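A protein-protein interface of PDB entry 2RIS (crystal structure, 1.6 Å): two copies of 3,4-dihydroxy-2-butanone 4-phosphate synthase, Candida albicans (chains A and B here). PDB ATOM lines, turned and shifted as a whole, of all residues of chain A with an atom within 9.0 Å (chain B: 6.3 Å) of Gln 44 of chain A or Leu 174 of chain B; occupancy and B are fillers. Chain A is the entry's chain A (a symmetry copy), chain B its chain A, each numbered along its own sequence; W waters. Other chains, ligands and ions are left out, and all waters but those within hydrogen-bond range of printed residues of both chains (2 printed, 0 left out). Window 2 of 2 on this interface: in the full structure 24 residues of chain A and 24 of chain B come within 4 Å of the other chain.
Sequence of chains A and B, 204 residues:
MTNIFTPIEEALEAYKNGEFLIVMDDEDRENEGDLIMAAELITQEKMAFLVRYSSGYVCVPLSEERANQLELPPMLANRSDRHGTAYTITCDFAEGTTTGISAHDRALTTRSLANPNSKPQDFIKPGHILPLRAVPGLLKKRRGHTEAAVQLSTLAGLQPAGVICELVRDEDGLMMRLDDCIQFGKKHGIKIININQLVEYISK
No position is printed for both chains.
Hydrophobic or aromatic side chains of chain A within 4 Å of the printed part of chain B: Ala 48 and Ile 101.
Along chain A the printed residues that touch a printed residue of chain B span positions 44 to 101.
Printed residues of chain B that touch a printed residue of chain A: Asp 170, Asp 172, Leu 174 and Met 175.
Hydrophobic or aromatic side chains of chain B that line the printed part of chain A: Leu 174 and Met 175.
Among the printed residues, 5 pairs touch across the chains.
Among the printed residues, Asp or Glu carboxylates within 4 Å of a Lys or Arg side-chain nitrogen of the other chain: Arg 52 of chain A with Asp 170 of chain B (3.8 Å).
Water W2 lies within hydrogen-bond range of the side-chain amide nitrogen of Gln 44 of chain A (2.7 Å) and the backbone carbonyl oxygen of Asp 172 of chain B (2.8 Å).
Water W1 lies within hydrogen-bond range of O of Gly 173 of chain B (2.8 Å), N of Ala 103 of chain A (2.9 Å) and SD of Met 175 of chain B (3.5 Å).
Thr 43 of chain A touches none of the printed residues of chain B.
Gln 44 of chain A touches two residues of chain B.
Of the printed residues of chain B, Ala 48 of chain A touches Asp 172.
Printed residues of chain B within 4 Å of Arg 52 of chain A: Asp 170 (3.8 Å).
Of the printed residues of chain B, Ile 101 of chain A touches Met 175 (3.7 Å).
Arg 111 of chain A touches none of the printed residues of chain B.
Of the printed residues of chain A, Asp 170 of chain B touches Arg 52 (3.8 Å).
No residue of chain A comes within 4 Å of Gly 173 of chain B.
Printed residues of chain A within 4 Å of Met 175 of chain B: Ile 101 (3.7 Å).
The nearest residue of chain B that does not touch Gln 44 of chain A is Gly 173 of chain B (5.1 Å).
The nearest printed residue of chain A that does not touch Asp 170 of chain B is Ala 48 of chain A (6.5 Å).
The side-chain carboxylate of Asp 170 of chain B lies within salt-bridge range of the guanidinium group of Arg 52 of chain A (3.8 Å).
Among the printed residues, pairs that only touch across the chains: Ala 48 of chain A with Asp 172 of chain B (3.6 Å), Gln 44 of chain A with Asp 172 of chain B (3.6 Å), Gln 44 of chain A with Leu 174 of chain B (3.6 Å) and Ile 101 of chain A with Met 175 of chain B (3.7 Å).
The guanidinium group (NE) of Arg 169 of chain B lies within salt-bridge range of the side-chain carboxylate (OD1) of Asp 172 of chain B.
The backbone NH (N) of Arg 169 of chain B lies within hydrogen-bond range of the backbone carbonyl oxygen (O) of Leu 174 of chain B (2.8 Å).
The side-chain carboxylate of Asp 172 of chain B sits close to the backbone NH of Leu 174 of chain B.
The backbone carbonyl oxygen (O) of Ile 101 of chain A lies within hydrogen-bond range of the guanidinium group (NE) of Arg 106 of chain A, at 3.3 Å.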
ATOM      1  N   PHE A  20     -24.955 -35.583 -27.678  1.00  0.00           N
ATOM      2  CA  PHE A  20     -26.056 -34.898 -28.333  1.00  0.00           C
ATOM      3  C   PHE A  20     -26.619 -35.793 -29.417  1.00  0.00           C
ATOM      4  O   PHE A  20     -25.920 -36.675 -29.954  1.00  0.00           O
ATOM      5  CB  PHE A  20     -25.568 -33.622 -29.016  1.00  0.00           C
ATOM      6  CG  PHE A  20     -25.248 -32.501 -28.071  1.00  0.00           C
ATOM      7  CD1 PHE A  20     -23.925 -32.185 -27.773  1.00  0.00           C
ATOM      8  CD2 PHE A  20     -26.259 -31.738 -27.500  1.00  0.00           C
ATOM      9  CE1 PHE A  20     -23.610 -31.130 -26.903  1.00  0.00           C
ATOM     10  CE2 PHE A  20     -25.952 -30.685 -26.635  1.00  0.00           C
ATOM     11  CZ  PHE A  20     -24.620 -30.379 -26.341  1.00  0.00           C
ATOM     12  N   MET A  37     -29.714 -33.076 -25.787  1.00  0.00           N
ATOM     13  CA  MET A  37     -29.060 -34.099 -24.957  1.00  0.00           C
ATOM     14  C   MET A  37     -29.731 -34.195 -23.597  1.00  0.00           C
ATOM     15  O   MET A  37     -30.581 -33.373 -23.263  1.00  0.00           O
ATOM     16  CB  MET A  37     -27.546 -33.862 -24.824  1.00  0.00           C
ATOM     17  CG  MET A  37     -27.119 -32.670 -23.958  1.00  0.00           C
ATOM     18  SD  MET A  37     -25.373 -32.753 -23.496  1.00  0.00           S
ATOM     19  CE  MET A  37     -25.396 -34.127 -22.328  1.00  0.00           C
ATOM     20  N   LEU A  41     -26.774 -34.768 -17.849  1.00  0.00           N
ATOM     21  CA  LEU A  41     -25.438 -35.125 -18.332  1.00  0.00           C
ATOM     22  C   LEU A  41     -24.665 -33.966 -18.953  1.00  0.00           C
ATOM     23  O   LEU A  41     -23.494 -34.131 -19.324  1.00  0.00           O
ATOM     24  CB  LEU A  41     -25.532 -36.294 -19.329  1.00  0.00           C
ATOM     25  CG  LEU A  41     -26.130 -37.611 -18.803  1.00  0.00           C
ATOM     26  CD1 LEU A  41     -26.199 -38.675 -19.897  1.00  0.00           C
ATOM     27  CD2 LEU A  41     -25.333 -38.128 -17.629  1.00  0.00           C
ATOM     28  N   ILE A  42     -25.314 -32.806 -19.084  1.00  0.00           N
ATOM     29  CA  ILE A  42     -24.653 -31.664 -19.711  1.00  0.00           C
ATOM     30  C   ILE A  42     -23.605 -31.004 -18.821  1.00  0.00           C
ATOM     31  O   ILE A  42     -23.899 -30.487 -17.741  1.00  0.00           O
ATOM     32  CB  ILE A  42     -25.656 -30.639 -20.326  1.00  0.00           C
ATOM     33  CG1 ILE A  42     -24.921 -29.660 -21.261  1.00  0.00           C
ATOM     34  CG2 ILE A  42     -26.475 -29.936 -19.239  1.00  0.00           C
ATOM     35  CD1 ILE A  42     -25.819 -28.999 -22.302  1.00  0.00           C
ATOM     36  N   THR A  43     -22.368 -31.037 -19.316  1.00  0.00           N
ATOM     37  CA  THR A  43     -21.213 -30.470 -18.631  1.00  0.00           C
ATOM     38  C   THR A  43     -20.992 -29.022 -19.072  1.00  0.00           C
ATOM     39  O   THR A  43     -21.594 -28.565 -20.046  1.00  0.00           O
ATOM     40  CB  THR A  43     -19.938 -31.267 -18.977  1.00  0.00           C
ATOM     41  OG1 THR A  43     -19.760 -31.260 -20.398  1.00  0.00           O
ATOM     42  CG2 THR A  43     -20.042 -32.712 -18.487  1.00  0.00           C
ATOM     43  N   GLN A  44     -20.112 -28.308 -18.368  1.00  0.00           N
ATOM     44  CA  GLN A  44     -19.658 -26.983 -18.794  1.00  0.00           C
ATOM     45  C   GLN A  44     -19.245 -26.993 -20.265  1.00  0.00           C
ATOM     46  O   GLN A  44     -19.676 -26.145 -21.033  1.00  0.00           O
ATOM     47  CB  GLN A  44     -18.471 -26.524 -17.928  1.00  0.00           C
ATOM     48  CG  GLN A  44     -18.075 -25.043 -18.085  1.00  0.00           C
ATOM     49  CD  GLN A  44     -17.154 -24.742 -19.266  1.00  0.00           C
ATOM     50  OE1 GLN A  44     -16.996 -23.573 -19.654  1.00  0.00           O
ATOM     51  NE2 GLN A  44     -16.536 -25.775 -19.831  1.00  0.00           N
ATOM     52  N   GLU A  45     -18.426 -27.975 -20.634  1.00  0.00           N
ATOM     53  CA  GLU A  45     -17.879 -28.087 -21.985  1.00  0.00           C
ATOM     54  C   GLU A  45     -18.979 -28.349 -23.002  1.00  0.00           C
ATOM     55  O   GLU A  45     -18.993 -27.741 -24.070  1.00  0.00           O
ATOM     56  CB  GLU A  45     -16.836 -29.205 -22.057  1.00  0.00           C
ATOM     57  CG  GLU A  45     -15.572 -28.944 -21.241  1.00  0.00           C
ATOM     58  CD  GLU A  45     -15.736 -29.156 -19.732  1.00  0.00           C
ATOM     59  OE1 GLU A  45     -16.763 -29.709 -19.269  1.00  0.00           O
ATOM     60  OE2 GLU A  45     -14.795 -28.766 -18.999  1.00  0.00           O
ATOM     61  N   LYS A  46     -19.918 -29.233 -22.656  1.00  0.00           N
ATOM     62  CA  LYS A  46     -21.017 -29.554 -23.576  1.00  0.00           C
ATOM     63  C   LYS A  46     -21.979 -28.379 -23.744  1.00  0.00           C
ATOM     64  O   LYS A  46     -22.531 -28.167 -24.831  1.00  0.00           O
ATOM     65  CB  LYS A  46     -21.736 -30.838 -23.145  1.00  0.00           C
ATOM     66  CG  LYS A  46     -20.913 -32.085 -23.456  1.00  0.00           C
ATOM     67  CD  LYS A  46     -21.434 -33.322 -22.762  1.00  0.00           C
ATOM     68  CE  LYS A  46     -20.601 -34.541 -23.171  1.00  0.00           C
ATOM     69  NZ  LYS A  46     -21.029 -35.791 -22.496  1.00  0.00           N
ATOM     70  N   MET A  47     -22.174 -27.610 -22.673  1.00  0.00           N
ATOM     71  CA  MET A  47     -22.975 -26.373 -22.749  1.00  0.00           C
ATOM     72  C   MET A  47     -22.272 -25.319 -23.605  1.00  0.00           C
ATOM     73  O   MET A  47     -22.906 -24.616 -24.403  1.00  0.00           O
ATOM     74  CB  MET A  47     -23.253 -25.815 -21.346  1.00  0.00           C
ATOM     75  CG  MET A  47     -24.158 -24.577 -21.320  1.00  0.00           C
ATOM     76  SD  MET A  47     -25.810 -24.806 -22.046  1.00  0.00           S
ATOM     77  CE  MET A  47     -26.682 -25.667 -20.740  1.00  0.00           C
ATOM     78  N   ALA A  48     -20.959 -25.206 -23.428  1.00  0.00           N
ATOM     79  CA  ALA A  48     -20.162 -24.313 -24.253  1.00  0.00           C
ATOM     80  C   ALA A  48     -20.332 -24.653 -25.737  1.00  0.00           C
ATOM     81  O   ALA A  48     -20.515 -23.761 -26.566  1.00  0.00           O
ATOM     82  CB  ALA A  48     -18.694 -24.340 -23.841  1.00  0.00           C
ATOM     83  N   PHE A  49     -20.293 -25.951 -26.051  1.00  0.00           N
ATOM     84  CA  PHE A  49     -20.470 -26.446 -27.407  1.00  0.00           C
ATOM     85  C   PHE A  49     -21.876 -26.110 -27.921  1.00  0.00           C
ATOM     86  O   PHE A  49     -22.032 -25.551 -29.007  1.00  0.00           O
ATOM     87  CB  PHE A  49     -20.216 -27.956 -27.434  1.00  0.00           C
ATOM     88  CG  PHE A  49     -20.354 -28.574 -28.794  1.00  0.00           C
ATOM     89  CD1 PHE A  49     -19.243 -28.721 -29.630  1.00  0.00           C
ATOM     90  CD2 PHE A  49     -21.593 -29.028 -29.239  1.00  0.00           C
ATOM     91  CE1 PHE A  49     -19.380 -29.302 -30.904  1.00  0.00           C
ATOM     92  CE2 PHE A  49     -21.730 -29.622 -30.502  1.00  0.00           C
ATOM     93  CZ  PHE A  49     -20.617 -29.759 -31.325  1.00  0.00           C
ATOM     94  N   LEU A  50     -22.897 -26.424 -27.120  1.00  0.00           N
ATOM     95  CA  LEU A  50     -24.278 -26.113 -27.487  1.00  0.00           C
ATOM     96  C   LEU A  50     -24.447 -24.637 -27.827  1.00  0.00           C
ATOM     97  O   LEU A  50     -25.014 -24.296 -28.856  1.00  0.00           O
ATOM     98  CB  LEU A  50     -25.235 -26.500 -26.353  1.00  0.00           C
ATOM     99  CG  LEU A  50     -26.733 -26.283 -26.586  1.00  0.00           C
ATOM    100  CD1 LEU A  50     -27.179 -27.028 -27.850  1.00  0.00           C
ATOM    101  CD2 LEU A  50     -27.538 -26.776 -25.396  1.00  0.00           C
ATOM    102  N   VAL A  51     -23.962 -23.765 -26.947  1.00  0.00           N
ATOM    103  CA  VAL A  51     -24.104 -22.324 -27.154  1.00  0.00           C
ATOM    104  C   VAL A  51     -23.330 -21.869 -28.391  1.00  0.00           C
ATOM    105  O   VAL A  51     -23.825 -21.075 -29.187  1.00  0.00           O
ATOM    106  CB  VAL A  51     -23.654 -21.554 -25.894  1.00  0.00           C
ATOM    107  CG1 VAL A  51     -23.535 -20.065 -26.168  1.00  0.00           C
ATOM    108  CG2 VAL A  51     -24.644 -21.817 -24.762  1.00  0.00           C
ATOM    109  N   ARG A  52     -22.120 -22.395 -28.554  1.00  0.00           N
ATOM    110  CA  ARG A  52     -21.260 -22.002 -29.665  1.00  0.00           C
ATOM    111  C   ARG A  52     -21.934 -22.177 -31.018  1.00  0.00           C
ATOM    112  O   ARG A  52     -21.776 -21.330 -31.905  1.00  0.00           O
ATOM    113  CB  ARG A  52     -19.947 -22.783 -29.616  1.00  0.00           C
ATOM    114  CG  ARG A  52     -19.088 -22.717 -30.861  1.00  0.00           C
ATOM    115  CD  ARG A  52     -18.527 -21.321 -31.168  1.00  0.00           C
ATOM    116  NE  ARG A  52     -17.752 -21.377 -32.401  1.00  0.00           N
ATOM    117  CZ  ARG A  52     -18.275 -21.283 -33.622  1.00  0.00           C
ATOM    118  NH1 ARG A  52     -19.583 -21.086 -33.785  1.00  0.00           N
ATOM    119  NH2 ARG A  52     -17.485 -21.372 -34.688  1.00  0.00           N
ATOM    120  N   ILE A 101     -25.338 -16.961 -16.522  1.00  0.00           N
ATOM    121  CA  ILE A 101     -25.301 -17.063 -17.984  1.00  0.00           C
ATOM    122  C   ILE A 101     -24.069 -17.827 -18.505  1.00  0.00           C
ATOM    123  O   ILE A 101     -24.048 -18.301 -19.659  1.00  0.00           O
ATOM    124  CB  ILE A 101     -25.451 -15.648 -18.648  1.00  0.00           C
ATOM    125  CG1 ILE A 101     -25.647 -15.729 -20.173  1.00  0.00           C
ATOM    126  CG2 ILE A 101     -24.262 -14.752 -18.301  1.00  0.00           C
ATOM    127  CD1 ILE A 101     -26.909 -16.443 -20.619  1.00  0.00           C
ATOM    128  N   SER A 102     -23.042 -17.956 -17.665  1.00  0.00           N
ATOM    129  CA  SER A 102     -21.849 -18.700 -18.070  1.00  0.00           C
ATOM    130  C   SER A 102     -22.207 -20.129 -18.478  1.00  0.00           C
ATOM    131  O   SER A 102     -23.209 -20.687 -18.026  1.00  0.00           O
ATOM    132  CB  SER A 102     -20.811 -18.719 -16.951  1.00  0.00           C
ATOM    133  OG  SER A 102     -21.251 -19.524 -15.868  1.00  0.00           O
ATOM    134  N   ALA A 103     -21.382 -20.726 -19.330  1.00  0.00           N
ATOM    135  CA  ALA A 103     -21.571 -22.140 -19.677  1.00  0.00           C
ATOM    136  C   ALA A 103     -21.628 -23.020 -18.422  1.00  0.00           C
ATOM    137  O   ALA A 103     -22.461 -23.917 -18.319  1.00  0.00           O
ATOM    138  CB  ALA A 103     -20.470 -22.597 -20.609  1.00  0.00           C
ATOM    139  N   HIS A 104     -20.728 -22.747 -17.478  1.00  0.00           N
ATOM    140  CA  HIS A 104     -20.697 -23.474 -16.212  1.00  0.00           C
ATOM    141  C   HIS A 104     -22.041 -23.373 -15.493  1.00  0.00           C
ATOM    142  O   HIS A 104     -22.598 -24.383 -15.033  1.00  0.00           O
ATOM    143  CB  HIS A 104     -19.591 -22.913 -15.322  1.00  0.00           C
ATOM    144  CG  HIS A 104     -19.651 -23.405 -13.911  1.00  0.00           C
ATOM    145  ND1 HIS A 104     -20.458 -22.824 -12.957  1.00  0.00           N
ATOM    146  CD2 HIS A 104     -19.011 -24.424 -13.296  1.00  0.00           C
ATOM    147  CE1 HIS A 104     -20.306 -23.461 -11.808  1.00  0.00           C
ATOM    148  NE2 HIS A 104     -19.434 -24.434 -11.988  1.00  0.00           N
ATOM    149  N   ASP A 105     -22.545 -22.146 -15.376  1.00  0.00           N
ATOM    150  CA  ASP A 105     -23.770 -21.908 -14.626  1.00  0.00           C
ATOM    151  C   ASP A 105     -24.993 -22.498 -15.323  1.00  0.00           C
ATOM    152  O   ASP A 105     -25.817 -23.159 -14.679  1.00  0.00           O
ATOM    153  CB  ASP A 105     -23.961 -20.415 -14.373  1.00  0.00           C
ATOM    154  CG  ASP A 105     -22.978 -19.855 -13.349  1.00  0.00           C
ATOM    155  OD1 ASP A 105     -22.068 -20.590 -12.875  1.00  0.00           O
ATOM    156  OD2 ASP A 105     -23.139 -18.660 -13.014  1.00  0.00           O
ATOM    157  N   ARG A 106     -25.118 -22.264 -16.632  1.00  0.00           N
ATOM    158  CA  ARG A 106     -26.244 -22.837 -17.379  1.00  0.00           C
ATOM    159  C   ARG A 106     -26.244 -24.366 -17.345  1.00  0.00           C
ATOM    160  O   ARG A 106     -27.303 -24.989 -17.225  1.00  0.00           O
ATOM    161  CB  ARG A 106     -26.318 -22.299 -18.813  1.00  0.00           C
ATOM    162  CG  ARG A 106     -26.837 -20.879 -18.863  1.00  0.00           C
ATOM    163  CD  ARG A 106     -27.433 -20.551 -20.207  1.00  0.00           C
ATOM    164  NE  ARG A 106     -26.422 -20.056 -21.146  1.00  0.00           N
ATOM    165  CZ  ARG A 106     -26.711 -19.565 -22.353  1.00  0.00           C
ATOM    166  NH1 ARG A 106     -27.974 -19.532 -22.786  1.00  0.00           N
ATOM    167  NH2 ARG A 106     -25.735 -19.114 -23.138  1.00  0.00           N
ATOM    168  N   ALA A 107     -25.058 -24.964 -17.427  1.00  0.00           N
ATOM    169  CA  ALA A 107     -24.945 -26.420 -17.311  1.00  0.00           C
ATOM    170  C   ALA A 107     -25.377 -26.881 -15.922  1.00  0.00           C
ATOM    171  O   ALA A 107     -26.152 -27.825 -15.797  1.00  0.00           O
ATOM    172  CB  ALA A 107     -23.526 -26.880 -17.612  1.00  0.00           C
ATOM    173  N   LEU A 108     -24.906 -26.182 -14.887  1.00  0.00           N
ATOM    174  CA  LEU A 108     -25.236 -26.554 -13.508  1.00  0.00           C
ATOM    175  C   LEU A 108     -26.737 -26.447 -13.269  1.00  0.00           C
ATOM    176  O   LEU A 108     -27.335 -27.326 -12.659  1.00  0.00           O
ATOM    177  CB  LEU A 108     -24.450 -25.698 -12.503  1.00  0.00           C
ATOM    178  CG  LEU A 108     -24.785 -25.801 -11.008  1.00  0.00           C
ATOM    179  CD1 LEU A 108     -24.624 -27.235 -10.494  1.00  0.00           C
ATOM    180  CD2 LEU A 108     -23.909 -24.859 -10.192  1.00  0.00           C
ATOM    181  N   ARG A 111     -28.484 -29.424 -15.132  1.00  0.00           N
ATOM    182  CA  ARG A 111     -28.327 -30.686 -14.397  1.00  0.00           C
ATOM    183  C   ARG A 111     -29.220 -30.671 -13.158  1.00  0.00           C
ATOM    184  O   ARG A 111     -29.850 -31.675 -12.820  1.00  0.00           O
ATOM    185  CB  ARG A 111     -26.866 -30.920 -13.999  1.00  0.00           C
ATOM    186  CG  ARG A 111     -25.940 -31.165 -15.193  1.00  0.00           C
ATOM    187  CD  ARG A 111     -24.603 -31.746 -14.735  1.00  0.00           C
ATOM    188  NE  ARG A 111     -23.987 -30.925 -13.689  1.00  0.00           N
ATOM    189  CZ  ARG A 111     -23.265 -29.826 -13.921  1.00  0.00           C
ATOM    190  NH1 ARG A 111     -23.068 -29.401 -15.168  1.00  0.00           N
ATOM    191  NH2 ARG A 111     -22.745 -29.142 -12.898  1.00  0.00           N
ATOM    192  N   LEU B 167     -20.319 -11.155 -24.622  1.00  0.00           N
ATOM    193  CA  LEU B 167     -19.284 -11.747 -25.475  1.00  0.00           C
ATOM    194  C   LEU B 167     -18.752 -13.044 -24.885  1.00  0.00           C
ATOM    195  O   LEU B 167     -18.484 -13.118 -23.682  1.00  0.00           O
ATOM    196  CB  LEU B 167     -18.128 -10.759 -25.677  1.00  0.00           C
ATOM    197  CG  LEU B 167     -18.422  -9.645 -26.684  1.00  0.00           C
ATOM    198  CD1 LEU B 167     -17.463  -8.493 -26.461  1.00  0.00           C
ATOM    199  CD2 LEU B 167     -18.338 -10.171 -28.131  1.00  0.00           C
ATOM    200  N   VAL B 168     -18.631 -14.064 -25.737  1.00  0.00           N
ATOM    201  CA  VAL B 168     -18.080 -15.362 -25.317  1.00  0.00           C
ATOM    202  C   VAL B 168     -16.973 -15.842 -26.247  1.00  0.00           C
ATOM    203  O   VAL B 168     -17.037 -15.635 -27.481  1.00  0.00           O
ATOM    204  CB  VAL B 168     -19.167 -16.463 -25.181  1.00  0.00           C
ATOM    205  CG1 VAL B 168     -20.269 -16.029 -24.241  1.00  0.00           C
ATOM    206  CG2 VAL B 168     -19.739 -16.870 -26.521  1.00  0.00           C
ATOM    207  N   ARG B 169     -15.974 -16.496 -25.659  1.00  0.00           N
ATOM    208  CA  ARG B 169     -14.827 -17.011 -26.410  1.00  0.00           C
ATOM    209  C   ARG B 169     -15.202 -18.239 -27.233  1.00  0.00           C
ATOM    210  O   ARG B 169     -15.855 -19.149 -26.731  1.00  0.00           O
ATOM    211  CB  ARG B 169     -13.689 -17.374 -25.449  1.00  0.00           C
ATOM    212  CG  ARG B 169     -13.088 -16.164 -24.726  1.00  0.00           C
ATOM    213  CD  ARG B 169     -12.362 -16.568 -23.448  1.00  0.00           C
ATOM    214  NE  ARG B 169     -11.529 -17.752 -23.636  1.00  0.00           N
ATOM    215  CZ  ARG B 169     -10.311 -17.752 -24.182  1.00  0.00           C
ATOM    216  NH1 ARG B 169      -9.648 -18.896 -24.312  1.00  0.00           N
ATOM    217  NH2 ARG B 169      -9.750 -16.621 -24.599  1.00  0.00           N
ATOM    218  N   ASP B 170     -14.759 -18.278 -28.488  1.00  0.00           N
ATOM    219  CA  ASP B 170     -14.968 -19.462 -29.329  1.00  0.00           C
ATOM    220  C   ASP B 170     -14.278 -20.717 -28.776  1.00  0.00           C
ATOM    221  O   ASP B 170     -14.774 -21.841 -28.950  1.00  0.00           O
ATOM    222  CB  ASP B 170     -14.434 -19.231 -30.748  1.00  0.00           C
ATOM    223  CG  ASP B 170     -15.369 -18.410 -31.615  1.00  0.00           C
ATOM    224  OD1 ASP B 170     -16.487 -18.061 -31.172  1.00  0.00           O
ATOM    225  OD2 ASP B 170     -14.965 -18.126 -32.763  1.00  0.00           O
ATOM    226  N   GLU B 171     -13.118 -20.521 -28.153  1.00  0.00           N
ATOM    227  CA  GLU B 171     -12.270 -21.642 -27.742  1.00  0.00           C
ATOM    228  C   GLU B 171     -12.936 -22.523 -26.695  1.00  0.00           C
ATOM    229  O   GLU B 171     -12.836 -23.755 -26.749  1.00  0.00           O
ATOM    230  CB  GLU B 171     -10.918 -21.150 -27.229  1.00  0.00           C
ATOM    231  CG  GLU B 171     -10.044 -20.532 -28.314  1.00  0.00           C
ATOM    232  CD  GLU B 171     -10.265 -19.040 -28.497  1.00  0.00           C
ATOM    233  OE1 GLU B 171     -11.256 -18.491 -27.956  1.00  0.00           O
ATOM    234  OE2 GLU B 171      -9.431 -18.413 -29.197  1.00  0.00           O
ATOM    235  N   ASP B 172     -13.632 -21.894 -25.751  1.00  0.00           N
ATOM    236  CA  ASP B 172     -14.059 -22.611 -24.558  1.00  0.00           C
ATOM    237  C   ASP B 172     -15.343 -22.092 -23.934  1.00  0.00           C
ATOM    238  O   ASP B 172     -15.750 -22.586 -22.879  1.00  0.00           O
ATOM    239  CB  ASP B 172     -12.948 -22.595 -23.498  1.00  0.00           C
ATOM    240  CG  ASP B 172     -12.378 -21.196 -23.252  1.00  0.00           C
ATOM    241  OD1 ASP B 172     -13.081 -20.197 -23.507  1.00  0.00           O
ATOM    242  OD2 ASP B 172     -11.217 -21.106 -22.791  1.00  0.00           O
ATOM    243  N   GLY B 173     -15.957 -21.094 -24.569  1.00  0.00           N
ATOM    244  CA  GLY B 173     -17.252 -20.584 -24.117  1.00  0.00           C
ATOM    245  C   GLY B 173     -17.185 -19.685 -22.893  1.00  0.00           C
ATOM    246  O   GLY B 173     -18.223 -19.270 -22.371  1.00  0.00           O
ATOM    247  N   LEU B 174     -15.970 -19.385 -22.435  1.00  0.00           N
ATOM    248  CA  LEU B 174     -15.791 -18.476 -21.304  1.00  0.00           C
ATOM    249  C   LEU B 174     -16.073 -17.038 -21.750  1.00  0.00           C
ATOM    250  O   LEU B 174     -15.816 -16.679 -22.897  1.00  0.00           O
ATOM    251  CB  LEU B 174     -14.377 -18.615 -20.729  1.00  0.00           C
ATOM    252  CG  LEU B 174     -13.986 -19.997 -20.193  1.00  0.00           C
ATOM    253  CD1 LEU B 174     -12.614 -19.896 -19.534  1.00  0.00           C
ATOM    254  CD2 LEU B 174     -15.010 -20.591 -19.223  1.00  0.00           C
ATOM    255  N   MET B 175     -16.641 -16.235 -20.855  1.00  0.00           N
ATOM    256  CA  MET B 175     -16.961 -14.850 -21.215  1.00  0.00           C
ATOM    257  C   MET B 175     -15.681 -14.053 -21.437  1.00  0.00           C
ATOM    258  O   MET B 175     -14.670 -14.295 -20.764  1.00  0.00           O
ATOM    259  CB  MET B 175     -17.849 -14.189 -20.162  1.00  0.00           C
ATOM    260  CG  MET B 175     -19.344 -14.333 -20.483  1.00  0.00           C
ATOM    261  SD  MET B 175     -19.929 -16.037 -20.411  1.00  0.00           S
ATOM    262  CE  MET B 175     -21.611 -15.819 -21.013  1.00  0.00           C
ATOM    263  N   MET B 176     -15.721 -13.108 -22.375  1.00  0.00           N
ATOM    264  CA  MET B 176     -14.524 -12.342 -22.706  1.00  0.00           C
ATOM    265  C   MET B 176     -14.255 -11.277 -21.654  1.00  0.00           C
ATOM    266  O   MET B 176     -15.093 -10.406 -21.430  1.00  0.00           O
ATOM    267  CB  MET B 176     -14.657 -11.678 -24.081  1.00  0.00           C
ATOM    268  CG  MET B 176     -14.538 -12.622 -25.247  1.00  0.00           C
ATOM    269  SD  MET B 176     -14.508 -11.716 -26.800  1.00  0.00           S
ATOM    270  CE  MET B 176     -14.926 -13.011 -27.963  1.00  0.00           C
ATOM    271  N   ARG B 177     -13.091 -11.374 -21.010  1.00  0.00           N
ATOM    272  CA  ARG B 177     -12.559 -10.331 -20.127  1.00  0.00           C
ATOM    273  C   ARG B 177     -11.948  -9.209 -20.980  1.00  0.00           C
ATOM    274  O   ARG B 177     -11.946  -9.283 -22.215  1.00  0.00           O
ATOM    275  CB  ARG B 177     -11.487 -10.935 -19.191  1.00  0.00           C
ATOM    276  CG  ARG B 177     -11.934 -11.433 -17.806  1.00  0.00           C
ATOM    277  CD  ARG B 177     -13.180 -12.257 -17.829  1.00  0.00           C
ATOM    278  NE  ARG B 177     -13.169 -13.414 -16.917  1.00  0.00           N
ATOM    279  CZ  ARG B 177     -13.541 -13.403 -15.637  1.00  0.00           C
ATOM    280  NH1 ARG B 177     -13.916 -12.278 -15.034  1.00  0.00           N
ATOM    281  NH2 ARG B 177     -13.525 -14.536 -14.944  1.00  0.00           N
ATOM    282  N   ASP B 180      -9.432  -9.934 -24.062  1.00  0.00           N
ATOM    283  CA  ASP B 180     -10.133 -10.534 -25.192  1.00  0.00           C
ATOM    284  C   ASP B 180     -11.072  -9.535 -25.870  1.00  0.00           C
ATOM    285  O   ASP B 180     -11.233  -9.566 -27.089  1.00  0.00           O
ATOM    286  CB  ASP B 180     -10.882 -11.807 -24.784  1.00  0.00           C
ATOM    287  CG  ASP B 180      -9.969 -13.030 -24.710  1.00  0.00           C
ATOM    288  OD1 ASP B 180     -10.376 -14.016 -24.062  1.00  0.00           O
ATOM    289  OD2 ASP B 180      -8.850 -13.013 -25.288  1.00  0.00           O
HETATM  290  O   HOH W   1     -18.861 -19.271 -19.686  1.00  0.00           O
HETATM  291  O   HOH W   2     -15.147 -25.175 -22.095  1.00  0.00           O
